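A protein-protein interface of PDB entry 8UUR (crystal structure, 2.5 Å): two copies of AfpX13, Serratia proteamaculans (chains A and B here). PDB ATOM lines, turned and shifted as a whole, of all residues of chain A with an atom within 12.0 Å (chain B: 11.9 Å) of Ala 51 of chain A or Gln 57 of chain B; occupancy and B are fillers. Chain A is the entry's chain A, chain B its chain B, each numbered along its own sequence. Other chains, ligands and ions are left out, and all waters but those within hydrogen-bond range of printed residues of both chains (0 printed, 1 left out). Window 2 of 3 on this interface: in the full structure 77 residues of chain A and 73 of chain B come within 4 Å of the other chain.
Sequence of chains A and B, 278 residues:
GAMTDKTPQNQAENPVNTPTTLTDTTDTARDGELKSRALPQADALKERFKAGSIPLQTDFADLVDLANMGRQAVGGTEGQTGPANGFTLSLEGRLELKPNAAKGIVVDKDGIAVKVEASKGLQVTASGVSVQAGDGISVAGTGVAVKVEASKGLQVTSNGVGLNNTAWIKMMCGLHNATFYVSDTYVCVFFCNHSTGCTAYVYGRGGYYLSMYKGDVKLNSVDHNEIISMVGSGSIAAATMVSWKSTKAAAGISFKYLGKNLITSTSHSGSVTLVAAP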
ATOM      1  N   ALA A  42       6.548  -5.130  34.157  1.00  0.00           N
ATOM      2  CA  ALA A  42       6.251  -6.550  34.006  1.00  0.00           C
ATOM      3  C   ALA A  42       4.875  -6.903  34.568  1.00  0.00           C
ATOM      4  O   ALA A  42       4.092  -7.604  33.913  1.00  0.00           O
ATOM      5  CB  ALA A  42       7.343  -7.394  34.681  1.00  0.00           C
ATOM      6  N   ASP A  43       4.575  -6.462  35.796  1.00  0.00           N
ATOM      7  CA  ASP A  43       3.289  -6.812  36.402  1.00  0.00           C
ATOM      8  C   ASP A  43       2.129  -6.204  35.612  1.00  0.00           C
ATOM      9  O   ASP A  43       1.187  -6.905  35.229  1.00  0.00           O
ATOM     10  CB  ASP A  43       3.254  -6.372  37.864  1.00  0.00           C
ATOM     11  CG  ASP A  43       3.682  -4.918  38.062  1.00  0.00           C
ATOM     12  OD1 ASP A  43       4.451  -4.392  37.230  1.00  0.00           O
ATOM     13  OD2 ASP A  43       3.246  -4.299  39.058  1.00  0.00           O
ATOM     14  N   ALA A  44       2.216  -4.911  35.308  1.00  0.00           N
ATOM     15  CA  ALA A  44       1.190  -4.268  34.494  1.00  0.00           C
ATOM     16  C   ALA A  44       0.979  -5.019  33.185  1.00  0.00           C
ATOM     17  O   ALA A  44      -0.157  -5.342  32.817  1.00  0.00           O
ATOM     18  CB  ALA A  44       1.571  -2.814  34.239  1.00  0.00           C
ATOM     19  N   LEU A  45       2.067  -5.344  32.486  1.00  0.00           N
ATOM     20  CA  LEU A  45       1.927  -6.021  31.203  1.00  0.00           C
ATOM     21  C   LEU A  45       1.330  -7.408  31.388  1.00  0.00           C
ATOM     22  O   LEU A  45       0.458  -7.827  30.613  1.00  0.00           O
ATOM     23  CB  LEU A  45       3.277  -6.098  30.486  1.00  0.00           C
ATOM     24  CG  LEU A  45       3.277  -6.537  29.005  1.00  0.00           C
ATOM     25  CD1 LEU A  45       2.261  -5.750  28.170  1.00  0.00           C
ATOM     26  CD2 LEU A  45       4.673  -6.458  28.359  1.00  0.00           C
ATOM     27  N   LYS A  46       1.768  -8.129  32.419  1.00  0.00           N
ATOM     28  CA  LYS A  46       1.161  -9.430  32.699  1.00  0.00           C
ATOM     29  C   LYS A  46      -0.346  -9.305  32.782  1.00  0.00           C
ATOM     30  O   LYS A  46      -1.075 -10.200  32.356  1.00  0.00           O
ATOM     31  CB  LYS A  46       1.686 -10.005  34.016  1.00  0.00           C
ATOM     32  CG  LYS A  46       2.988 -10.716  33.913  1.00  0.00           C
ATOM     33  CD  LYS A  46       3.608 -10.883  35.298  1.00  0.00           C
ATOM     34  CE  LYS A  46       4.866 -11.700  35.236  1.00  0.00           C
ATOM     35  NZ  LYS A  46       5.163 -12.280  36.576  1.00  0.00           N
ATOM     36  N   GLU A  47      -0.821  -8.175  33.281  1.00  0.00           N
ATOM     37  CA  GLU A  47      -2.227  -8.055  33.609  1.00  0.00           C
ATOM     38  C   GLU A  47      -3.052  -8.057  32.335  1.00  0.00           C
ATOM     39  O   GLU A  47      -4.226  -8.438  32.346  1.00  0.00           O
ATOM     40  CB  GLU A  47      -2.452  -6.754  34.344  1.00  0.00           C
ATOM     41  CG  GLU A  47      -3.635  -6.721  35.243  1.00  0.00           C
ATOM     42  CD  GLU A  47      -3.858  -5.319  35.718  1.00  0.00           C
ATOM     43  OE1 GLU A  47      -3.356  -4.423  35.026  1.00  0.00           O
ATOM     44  OE2 GLU A  47      -4.285  -5.121  36.876  1.00  0.00           O
ATOM     45  N   ARG A  48      -2.438  -7.623  31.233  1.00  0.00           N
ATOM     46  CA  ARG A  48      -3.096  -7.535  29.941  1.00  0.00           C
ATOM     47  C   ARG A  48      -3.199  -8.888  29.256  1.00  0.00           C
ATOM     48  O   ARG A  48      -3.929  -9.012  28.269  1.00  0.00           O
ATOM     49  CB  ARG A  48      -2.329  -6.563  29.043  1.00  0.00           C
ATOM     50  CG  ARG A  48      -1.989  -5.242  29.681  1.00  0.00           C
ATOM     51  CD  ARG A  48      -3.234  -4.419  29.848  1.00  0.00           C
ATOM     52  NE  ARG A  48      -3.844  -4.142  28.561  1.00  0.00           N
ATOM     53  CZ  ARG A  48      -5.155  -4.019  28.364  1.00  0.00           C
ATOM     54  NH1 ARG A  48      -6.003  -4.145  29.370  1.00  0.00           N
ATOM     55  NH2 ARG A  48      -5.625  -3.763  27.158  1.00  0.00           N
ATOM     56  N   PHE A  49      -2.457  -9.886  29.732  1.00  0.00           N
ATOM     57  CA  PHE A  49      -2.548 -11.248  29.234  1.00  0.00           C
ATOM     58  C   PHE A  49      -3.099 -12.175  30.306  1.00  0.00           C
ATOM     59  O   PHE A  49      -2.699 -13.334  30.406  1.00  0.00           O
ATOM     60  CB  PHE A  49      -1.188 -11.734  28.753  1.00  0.00           C
ATOM     61  CG  PHE A  49      -0.636 -10.954  27.608  1.00  0.00           C
ATOM     62  CD1 PHE A  49      -0.934 -11.317  26.303  1.00  0.00           C
ATOM     63  CD2 PHE A  49       0.187  -9.856  27.832  1.00  0.00           C
ATOM     64  CE1 PHE A  49      -0.416 -10.595  25.222  1.00  0.00           C
ATOM     65  CE2 PHE A  49       0.706  -9.118  26.768  1.00  0.00           C
ATOM     66  CZ  PHE A  49       0.406  -9.490  25.453  1.00  0.00           C
ATOM     67  N   LYS A  50      -3.991 -11.650  31.137  1.00  0.00           N
ATOM     68  CA  LYS A  50      -4.584 -12.413  32.218  1.00  0.00           C
ATOM     69  C   LYS A  50      -5.649 -13.361  31.670  1.00  0.00           C
ATOM     70  O   LYS A  50      -6.156 -13.194  30.556  1.00  0.00           O
ATOM     71  CB  LYS A  50      -5.176 -11.468  33.264  1.00  0.00           C
ATOM     72  N   ALA A  51      -5.972 -14.378  32.469  1.00  0.00           N
ATOM     73  CA  ALA A  51      -7.001 -15.344  32.096  1.00  0.00           C
ATOM     74  C   ALA A  51      -8.287 -14.643  31.666  1.00  0.00           C
ATOM     75  O   ALA A  51      -8.798 -13.763  32.362  1.00  0.00           O
ATOM     76  CB  ALA A  51      -7.283 -16.288  33.270  1.00  0.00           C
ATOM     77  N   GLY A  52      -8.804 -15.030  30.507  1.00  0.00           N
ATOM     78  CA  GLY A  52     -10.014 -14.442  29.976  1.00  0.00           C
ATOM     79  C   GLY A  52      -9.833 -13.187  29.147  1.00  0.00           C
ATOM     80  O   GLY A  52     -10.829 -12.642  28.654  1.00  0.00           O
ATOM     81  N   SER A  53      -8.612 -12.697  28.971  1.00  0.00           N
ATOM     82  CA  SER A  53      -8.436 -11.430  28.279  1.00  0.00           C
ATOM     83  C   SER A  53      -8.252 -11.652  26.784  1.00  0.00           C
ATOM     84  O   SER A  53      -7.801 -12.715  26.343  1.00  0.00           O
ATOM     85  CB  SER A  53      -7.236 -10.661  28.835  1.00  0.00           C
ATOM     86  OG  SER A  53      -6.018 -11.249  28.404  1.00  0.00           O
ATOM     87  N   ILE A  54      -8.612 -10.630  26.010  1.00  0.00           N
ATOM     88  CA  ILE A  54      -8.348 -10.602  24.574  1.00  0.00           C
ATOM     89  C   ILE A  54      -7.288  -9.528  24.368  1.00  0.00           C
ATOM     90  O   ILE A  54      -7.617  -8.336  24.281  1.00  0.00           O
ATOM     91  CB  ILE A  54      -9.621 -10.328  23.755  1.00  0.00           C
ATOM     92  N   PRO A  55      -6.011  -9.901  24.338  1.00  0.00           N
ATOM     93  CA  PRO A  55      -4.952  -8.893  24.215  1.00  0.00           C
ATOM     94  C   PRO A  55      -5.083  -8.133  22.907  1.00  0.00           C
ATOM     95  O   PRO A  55      -5.396  -8.709  21.866  1.00  0.00           O
ATOM     96  CB  PRO A  55      -3.660  -9.721  24.266  1.00  0.00           C
ATOM     97  CG  PRO A  55      -4.049 -11.016  24.877  1.00  0.00           C
ATOM     98  CD  PRO A  55      -5.476 -11.264  24.485  1.00  0.00           C
ATOM     99  N   ASP A  59      -1.096  -4.300  23.202  1.00  0.00           N
ATOM    100  CA  ASP A  59      -0.476  -5.122  24.237  1.00  0.00           C
ATOM    101  C   ASP A  59       0.676  -5.923  23.648  1.00  0.00           C
ATOM    102  O   ASP A  59       1.773  -5.985  24.222  1.00  0.00           O
ATOM    103  CB  ASP A  59      -1.502  -6.057  24.875  1.00  0.00           C
ATOM    104  CG  ASP A  59      -2.682  -5.317  25.458  1.00  0.00           C
ATOM    105  OD1 ASP A  59      -2.495  -4.195  25.977  1.00  0.00           O
ATOM    106  OD2 ASP A  59      -3.803  -5.870  25.417  1.00  0.00           O
ATOM    107  N   PHE A  60       0.439  -6.522  22.480  1.00  0.00           N
ATOM    108  CA  PHE A  60       1.469  -7.273  21.784  1.00  0.00           C
ATOM    109  C   PHE A  60       2.596  -6.372  21.297  1.00  0.00           C
ATOM    110  O   PHE A  60       3.759  -6.788  21.279  1.00  0.00           O
ATOM    111  CB  PHE A  60       0.839  -8.025  20.621  1.00  0.00           C
ATOM    112  CG  PHE A  60       0.142  -9.274  21.032  1.00  0.00           C
ATOM    113  CD1 PHE A  60       0.869 -10.371  21.478  1.00  0.00           C
ATOM    114  CD2 PHE A  60      -1.243  -9.364  20.967  1.00  0.00           C
ATOM    115  CE1 PHE A  60       0.231 -11.531  21.858  1.00  0.00           C
ATOM    116  CE2 PHE A  60      -1.887 -10.523  21.340  1.00  0.00           C
ATOM    117  CZ  PHE A  60      -1.140 -11.614  21.795  1.00  0.00           C
ATOM    118  N   LEU A  63       4.765  -5.909  24.246  1.00  0.00           N
ATOM    119  CA  LEU A  63       5.548  -7.120  24.452  1.00  0.00           C
ATOM    120  C   LEU A  63       6.701  -7.233  23.457  1.00  0.00           C
ATOM    121  O   LEU A  63       7.830  -7.544  23.845  1.00  0.00           O
ATOM    122  CB  LEU A  63       4.635  -8.344  24.358  1.00  0.00           C
ATOM    123  CG  LEU A  63       5.240  -9.697  24.730  1.00  0.00           C
ATOM    124  CD1 LEU A  63       6.074  -9.599  25.996  1.00  0.00           C
ATOM    125  CD2 LEU A  63       4.133 -10.721  24.884  1.00  0.00           C
ATOM    126  N   LEU B  39      12.805 -18.638  34.738  1.00  0.00           N
ATOM    127  CA  LEU B  39      11.995 -18.712  33.541  1.00  0.00           C
ATOM    128  C   LEU B  39      12.357 -19.959  32.753  1.00  0.00           C
ATOM    129  O   LEU B  39      13.494 -20.426  32.815  1.00  0.00           O
ATOM    130  CB  LEU B  39      12.202 -17.469  32.679  1.00  0.00           C
ATOM    131  CG  LEU B  39      12.210 -16.205  33.545  1.00  0.00           C
ATOM    132  CD1 LEU B  39      12.375 -14.984  32.697  1.00  0.00           C
ATOM    133  CD2 LEU B  39      10.927 -16.107  34.354  1.00  0.00           C
ATOM    134  N   PRO B  40      11.396 -20.522  32.025  1.00  0.00           N
ATOM    135  CA  PRO B  40      11.700 -21.632  31.118  1.00  0.00           C
ATOM    136  C   PRO B  40      12.729 -21.230  30.074  1.00  0.00           C
ATOM    137  O   PRO B  40      12.908 -20.056  29.748  1.00  0.00           O
ATOM    138  CB  PRO B  40      10.353 -21.936  30.450  1.00  0.00           C
ATOM    139  CG  PRO B  40       9.340 -21.271  31.275  1.00  0.00           C
ATOM    140  CD  PRO B  40       9.970 -20.148  32.016  1.00  0.00           C
ATOM    141  N   LEU B  45       9.549 -22.775  26.317  1.00  0.00           N
ATOM    142  CA  LEU B  45       8.509 -21.765  26.235  1.00  0.00           C
ATOM    143  C   LEU B  45       7.801 -21.845  24.884  1.00  0.00           C
ATOM    144  O   LEU B  45       6.578 -21.650  24.802  1.00  0.00           O
ATOM    145  CB  LEU B  45       9.117 -20.383  26.493  1.00  0.00           C
ATOM    146  CG  LEU B  45       8.151 -19.221  26.766  1.00  0.00           C
ATOM    147  CD1 LEU B  45       7.096 -19.561  27.832  1.00  0.00           C
ATOM    148  CD2 LEU B  45       8.906 -17.914  27.100  1.00  0.00           C
ATOM    149  N   ARG B  48       4.846 -24.149  24.543  1.00  0.00           N
ATOM    150  CA  ARG B  48       3.641 -23.616  25.163  1.00  0.00           C
ATOM    151  C   ARG B  48       2.789 -22.821  24.175  1.00  0.00           C
ATOM    152  O   ARG B  48       1.602 -22.600  24.423  1.00  0.00           O
ATOM    153  CB  ARG B  48       4.032 -22.749  26.355  1.00  0.00           C
ATOM    154  CG  ARG B  48       4.842 -23.511  27.370  1.00  0.00           C
ATOM    155  CD  ARG B  48       4.012 -24.646  27.917  1.00  0.00           C
ATOM    156  NE  ARG B  48       2.796 -24.170  28.546  1.00  0.00           N
ATOM    157  CZ  ARG B  48       1.731 -24.920  28.758  1.00  0.00           C
ATOM    158  NH1 ARG B  48       1.731 -26.182  28.364  1.00  0.00           N
ATOM    159  NH2 ARG B  48       0.665 -24.408  29.358  1.00  0.00           N
ATOM    160  N   PHE B  49       3.370 -22.377  23.065  1.00  0.00           N
ATOM    161  CA  PHE B  49       2.665 -21.600  22.058  1.00  0.00           C
ATOM    162  C   PHE B  49       2.609 -22.379  20.752  1.00  0.00           C
ATOM    163  O   PHE B  49       2.573 -21.806  19.664  1.00  0.00           O
ATOM    164  CB  PHE B  49       3.340 -20.239  21.882  1.00  0.00           C
ATOM    165  CG  PHE B  49       3.220 -19.338  23.092  1.00  0.00           C
ATOM    166  CD1 PHE B  49       4.178 -19.360  24.089  1.00  0.00           C
ATOM    167  CD2 PHE B  49       2.126 -18.493  23.239  1.00  0.00           C
ATOM    168  CE1 PHE B  49       4.063 -18.534  25.215  1.00  0.00           C
ATOM    169  CE2 PHE B  49       1.993 -17.666  24.356  1.00  0.00           C
ATOM    170  CZ  PHE B  49       2.965 -17.684  25.352  1.00  0.00           C
ATOM    171  N   SER B  53      -2.135 -25.668  21.204  1.00  0.00           N
ATOM    172  CA  SER B  53      -1.842 -25.585  22.629  1.00  0.00           C
ATOM    173  C   SER B  53      -2.614 -24.426  23.243  1.00  0.00           C
ATOM    174  O   SER B  53      -2.833 -23.393  22.598  1.00  0.00           O
ATOM    175  CB  SER B  53      -0.348 -25.398  22.899  1.00  0.00           C
ATOM    176  OG  SER B  53      -0.108 -25.372  24.296  1.00  0.00           O
ATOM    177  N   ILE B  54      -3.031 -24.609  24.493  1.00  0.00           N
ATOM    178  CA  ILE B  54      -3.848 -23.616  25.186  1.00  0.00           C
ATOM    179  C   ILE B  54      -2.921 -22.728  26.000  1.00  0.00           C
ATOM    180  O   ILE B  54      -2.611 -23.055  27.156  1.00  0.00           O
ATOM    181  CB  ILE B  54      -4.905 -24.284  26.077  1.00  0.00           C
ATOM    182  N   PRO B  55      -2.447 -21.612  25.445  1.00  0.00           N
ATOM    183  CA  PRO B  55      -1.489 -20.778  26.179  1.00  0.00           C
ATOM    184  C   PRO B  55      -2.189 -20.133  27.369  1.00  0.00           C
ATOM    185  O   PRO B  55      -3.166 -19.398  27.209  1.00  0.00           O
ATOM    186  CB  PRO B  55      -1.045 -19.738  25.136  1.00  0.00           C
ATOM    187  CG  PRO B  55      -1.754 -20.096  23.860  1.00  0.00           C
ATOM    188  CD  PRO B  55      -2.937 -20.921  24.249  1.00  0.00           C
ATOM    189  N   LEU B  56      -1.698 -20.429  28.561  1.00  0.00           N
ATOM    190  CA  LEU B  56      -2.288 -19.900  29.778  1.00  0.00           C
ATOM    191  C   LEU B  56      -1.685 -18.548  30.136  1.00  0.00           C
ATOM    192  O   LEU B  56      -0.629 -18.145  29.642  1.00  0.00           O
ATOM    193  CB  LEU B  56      -2.097 -20.863  30.957  1.00  0.00           C
ATOM    194  CG  LEU B  56      -2.346 -22.351  30.703  1.00  0.00           C
ATOM    195  CD1 LEU B  56      -2.015 -23.201  31.935  1.00  0.00           C
ATOM    196  CD2 LEU B  56      -3.794 -22.552  30.283  1.00  0.00           C
ATOM    197  N   GLN B  57      -2.402 -17.843  30.997  1.00  0.00           N
ATOM    198  CA  GLN B  57      -1.887 -16.681  31.699  1.00  0.00           C
ATOM    199  C   GLN B  57      -0.435 -16.858  32.129  1.00  0.00           C
ATOM    200  O   GLN B  57       0.394 -15.961  31.959  1.00  0.00           O
ATOM    201  CB  GLN B  57      -2.809 -16.463  32.893  1.00  0.00           C
ATOM    202  CG  GLN B  57      -2.515 -15.364  33.849  1.00  0.00           C
ATOM    203  CD  GLN B  57      -3.498 -15.465  34.994  1.00  0.00           C
ATOM    204  OE1 GLN B  57      -4.005 -16.555  35.272  1.00  0.00           O
ATOM    205  NE2 GLN B  57      -3.787 -14.343  35.654  1.00  0.00           N
ATOM    206  N   THR B  58      -0.107 -18.025  32.677  1.00  0.00           N
ATOM    207  CA  THR B  58       1.233 -18.240  33.208  1.00  0.00           C
ATOM    208  C   THR B  58       2.259 -18.400  32.099  1.00  0.00           C
ATOM    209  O   THR B  58       3.442 -18.120  32.308  1.00  0.00           O
ATOM    210  CB  THR B  58       1.244 -19.472  34.110  1.00  0.00           C
ATOM    211  OG1 THR B  58       0.557 -20.542  33.451  1.00  0.00           O
ATOM    212  CG2 THR B  58       0.540 -19.176  35.411  1.00  0.00           C
ATOM    213  N   ASP B  59       1.835 -18.850  30.921  1.00  0.00           N
ATOM    214  CA  ASP B  59       2.747 -18.902  29.782  1.00  0.00           C
ATOM    215  C   ASP B  59       3.087 -17.508  29.293  1.00  0.00           C
ATOM    216  O   ASP B  59       4.262 -17.207  29.035  1.00  0.00           O
ATOM    217  CB  ASP B  59       2.126 -19.733  28.669  1.00  0.00           C
ATOM    218  CG  ASP B  59       1.856 -21.143  29.119  1.00  0.00           C
ATOM    219  OD1 ASP B  59       2.761 -21.750  29.748  1.00  0.00           O
ATOM    220  OD2 ASP B  59       0.732 -21.627  28.895  1.00  0.00           O
ATOM    221  N   PHE B  60       2.073 -16.638  29.183  1.00  0.00           N
ATOM    222  CA  PHE B  60       2.319 -15.232  28.884  1.00  0.00           C
ATOM    223  C   PHE B  60       3.099 -14.560  30.002  1.00  0.00           C
ATOM    224  O   PHE B  60       3.967 -13.718  29.746  1.00  0.00           O
ATOM    225  CB  PHE B  60       0.995 -14.504  28.628  1.00  0.00           C
ATOM    226  CG  PHE B  60       0.366 -14.835  27.290  1.00  0.00           C
ATOM    227  CD1 PHE B  60       0.760 -14.165  26.135  1.00  0.00           C
ATOM    228  CD2 PHE B  60      -0.609 -15.824  27.184  1.00  0.00           C
ATOM    229  CE1 PHE B  60       0.164 -14.468  24.891  1.00  0.00           C
ATOM    230  CE2 PHE B  60      -1.187 -16.137  25.957  1.00  0.00           C
ATOM    231  CZ  PHE B  60      -0.794 -15.457  24.806  1.00  0.00           C
ATOM    232  N   ALA B  61       2.817 -14.913  31.251  1.00  0.00           N
ATOM    233  CA  ALA B  61       3.596 -14.329  32.336  1.00  0.00           C
ATOM    234  C   ALA B  61       5.073 -14.655  32.161  1.00  0.00           C
ATOM    235  O   ALA B  61       5.944 -13.819  32.441  1.00  0.00           O
ATOM    236  CB  ALA B  61       3.088 -14.833  33.677  1.00  0.00           C
ATOM    237  N   ASP B  62       5.361 -15.857  31.646  1.00  0.00           N
ATOM    238  CA  ASP B  62       6.732 -16.302  31.421  1.00  0.00           C
ATOM    239  C   ASP B  62       7.369 -15.560  30.253  1.00  0.00           C
ATOM    240  O   ASP B  62       8.544 -15.188  30.301  1.00  0.00           O
ATOM    241  CB  ASP B  62       6.723 -17.808  31.183  1.00  0.00           C
ATOM    242  CG  ASP B  62       6.490 -18.600  32.468  1.00  0.00           C
ATOM    243  OD1 ASP B  62       6.540 -17.982  33.563  1.00  0.00           O
ATOM    244  OD2 ASP B  62       6.263 -19.834  32.377  1.00  0.00           O
ATOM    245  N   LEU B  63       6.592 -15.324  29.204  1.00  0.00           N
ATOM    246  CA  LEU B  63       7.052 -14.526  28.083  1.00  0.00           C
ATOM    247  C   LEU B  63       7.420 -13.109  28.516  1.00  0.00           C
ATOM    248  O   LEU B  63       8.499 -12.614  28.173  1.00  0.00           O
ATOM    249  CB  LEU B  63       5.962 -14.512  27.010  1.00  0.00           C
ATOM    250  CG  LEU B  63       6.377 -14.033  25.635  1.00  0.00           C
ATOM    251  CD1 LEU B  63       7.660 -14.747  25.237  1.00  0.00           C
ATOM    252  CD2 LEU B  63       5.252 -14.362  24.687  1.00  0.00           C
ATOM    253  N   VAL B  64       6.541 -12.448  29.280  1.00  0.00           N
ATOM    254  CA  VAL B  64       6.805 -11.079  29.746  1.00  0.00           C
ATOM    255  C   VAL B  64       8.093 -11.022  30.570  1.00  0.00           C
ATOM    256  O   VAL B  64       8.959 -10.155  30.355  1.00  0.00           O
ATOM    257  CB  VAL B  64       5.600 -10.539  30.554  1.00  0.00           C
ATOM    258  CG1 VAL B  64       5.997  -9.339  31.431  1.00  0.00           C
ATOM    259  CG2 VAL B  64       4.416 -10.153  29.638  1.00  0.00           C
ATOM    260  N   ASP B  65       8.231 -11.922  31.548  1.00  0.00           N
ATOM    261  CA  ASP B  65       9.415 -11.879  32.393  1.00  0.00           C
ATOM    262  C   ASP B  65      10.669 -12.190  31.584  1.00  0.00           C
ATOM    263  O   ASP B  65      11.724 -11.584  31.811  1.00  0.00           O
ATOM    264  CB  ASP B  65       9.268 -12.845  33.565  1.00  0.00           C
ATOM    265  CG  ASP B  65       8.352 -12.315  34.633  1.00  0.00           C
ATOM    266  OD1 ASP B  65       8.293 -11.081  34.785  1.00  0.00           O
ATOM    267  OD2 ASP B  65       7.685 -13.119  35.328  1.00  0.00           O
ATOM    268  N   LEU B  66      10.571 -13.131  30.638  1.00  0.00           N
ATOM    269  CA  LEU B  66      11.668 -13.370  29.711  1.00  0.00           C
ATOM    270  C   LEU B  66      12.043 -12.076  28.986  1.00  0.00           C
ATOM    271  O   LEU B  66      13.187 -11.624  29.064  1.00  0.00           O
ATOM    272  CB  LEU B  66      11.297 -14.489  28.724  1.00  0.00           C
ATOM    273  CG  LEU B  66      12.567 -14.871  27.943  1.00  0.00           C
ATOM    274  CD1 LEU B  66      13.865 -14.973  28.852  1.00  0.00           C
ATOM    275  CD2 LEU B  66      12.368 -16.155  27.148  1.00  0.00           C
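OD2 of Asp 65 of chain B is in salt-bridge range of NZ of Lys 46 of chain A (2.9 Å).
OG of Ser 53 of chain A lies within hydrogen-bond range of O of Lys 50 of chain A (2.9 Å).
Among the printed residues, merely in contact across the chains: Phe 49 of chain A with Phe 60 of chain B (3.3 Å), Ala 42 of chain A with Val 64 of chain B (3.6 Å), Lys 46 of chain A with Ala 61 of chain B (3.7 Å), Phe 49 of chain A with Gln 57 of chain B (3.7 Å), Ala 51 of chain A with Gln 57 of chain B (3.7 Å), Ala 42 of chain A with Asp 65 of chain B (3.8 Å), Leu 63 of chain A with Leu 63 of chain B (3.8 Å), Leu 45 of chain A with Val 64 of chain B (3.8 Å) and Lys 50 of chain A with Gln 57 of chain B (3.96 Å).
Ala 51 of chain A touches one residue of chain B. Gln 57 of chain B touches just these residues of chain A: Phe 49 (3.7 Å), Lys 50 (3.96 Å) and Ala 51 (3.7 Å). Printed residues of chain B within 4 Å of Lys 50 of chain A: Gln 57. Ser 53 of chain A touches none of the printed residues of chain B. No residue of chain A comes within 4 Å of Pro 55 of chain B. Leu 56 of chain B touches none of the printed residues of chain A. Thr 58 of chain B touches none of the printed residues of chain A. No residue of chain A comes within 4 Å of Asp 59 of chain B. Phe 60 of chain B touches one residue of chain A. Of the printed residues of chain B, Leu 45 of chain A touches Val 64. Printed residues of chain B within 4 Å of Ala 42 of chain A: Val 64 and Asp 65. Of the printed residues of chain A, Asp 65 of chain B touches Ala 42 (3.8 Å) and Lys 46 (2.9 Å). Printed residues of chain A within 4 Å of Leu 63 of chain B: Leu 63 (3.8 Å). Printed residues of chain B within 4 Å of Leu 63 of chain A: Leu 63. Ser 53 of chain B touches none of the printed residues of chain A. The nearest residue of chain B that does not touch Ala 51 of chain A is Leu 56 of chain B (6.4 Å). The nearest printed residue of chain B that does not touch Ala 42 of chain A is Ala 61 of chain B (6.7 Å).
Hydrophobic or aromatic side chains of chain B within 4 Å of the printed part of chain A: Phe 60, Ala 61, Leu 63 and Val 64. Of the 17 printed residues of chain A, 7 touch a printed residue of chain B. Hydrophobic or aromatic side chains of chain A that line the printed part of chain B: Ala 42, Leu 45, Phe 49, Ala 51 and Leu 63.
Phe 49 of chain A touches Phe 60 of chain B, but with the chains exchanged Phe 60 of chain A does not touch Phe 49 of chain B (6.9 Å). Leu 63 of chain B touches its own counterpart, Leu 63 of chain A.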
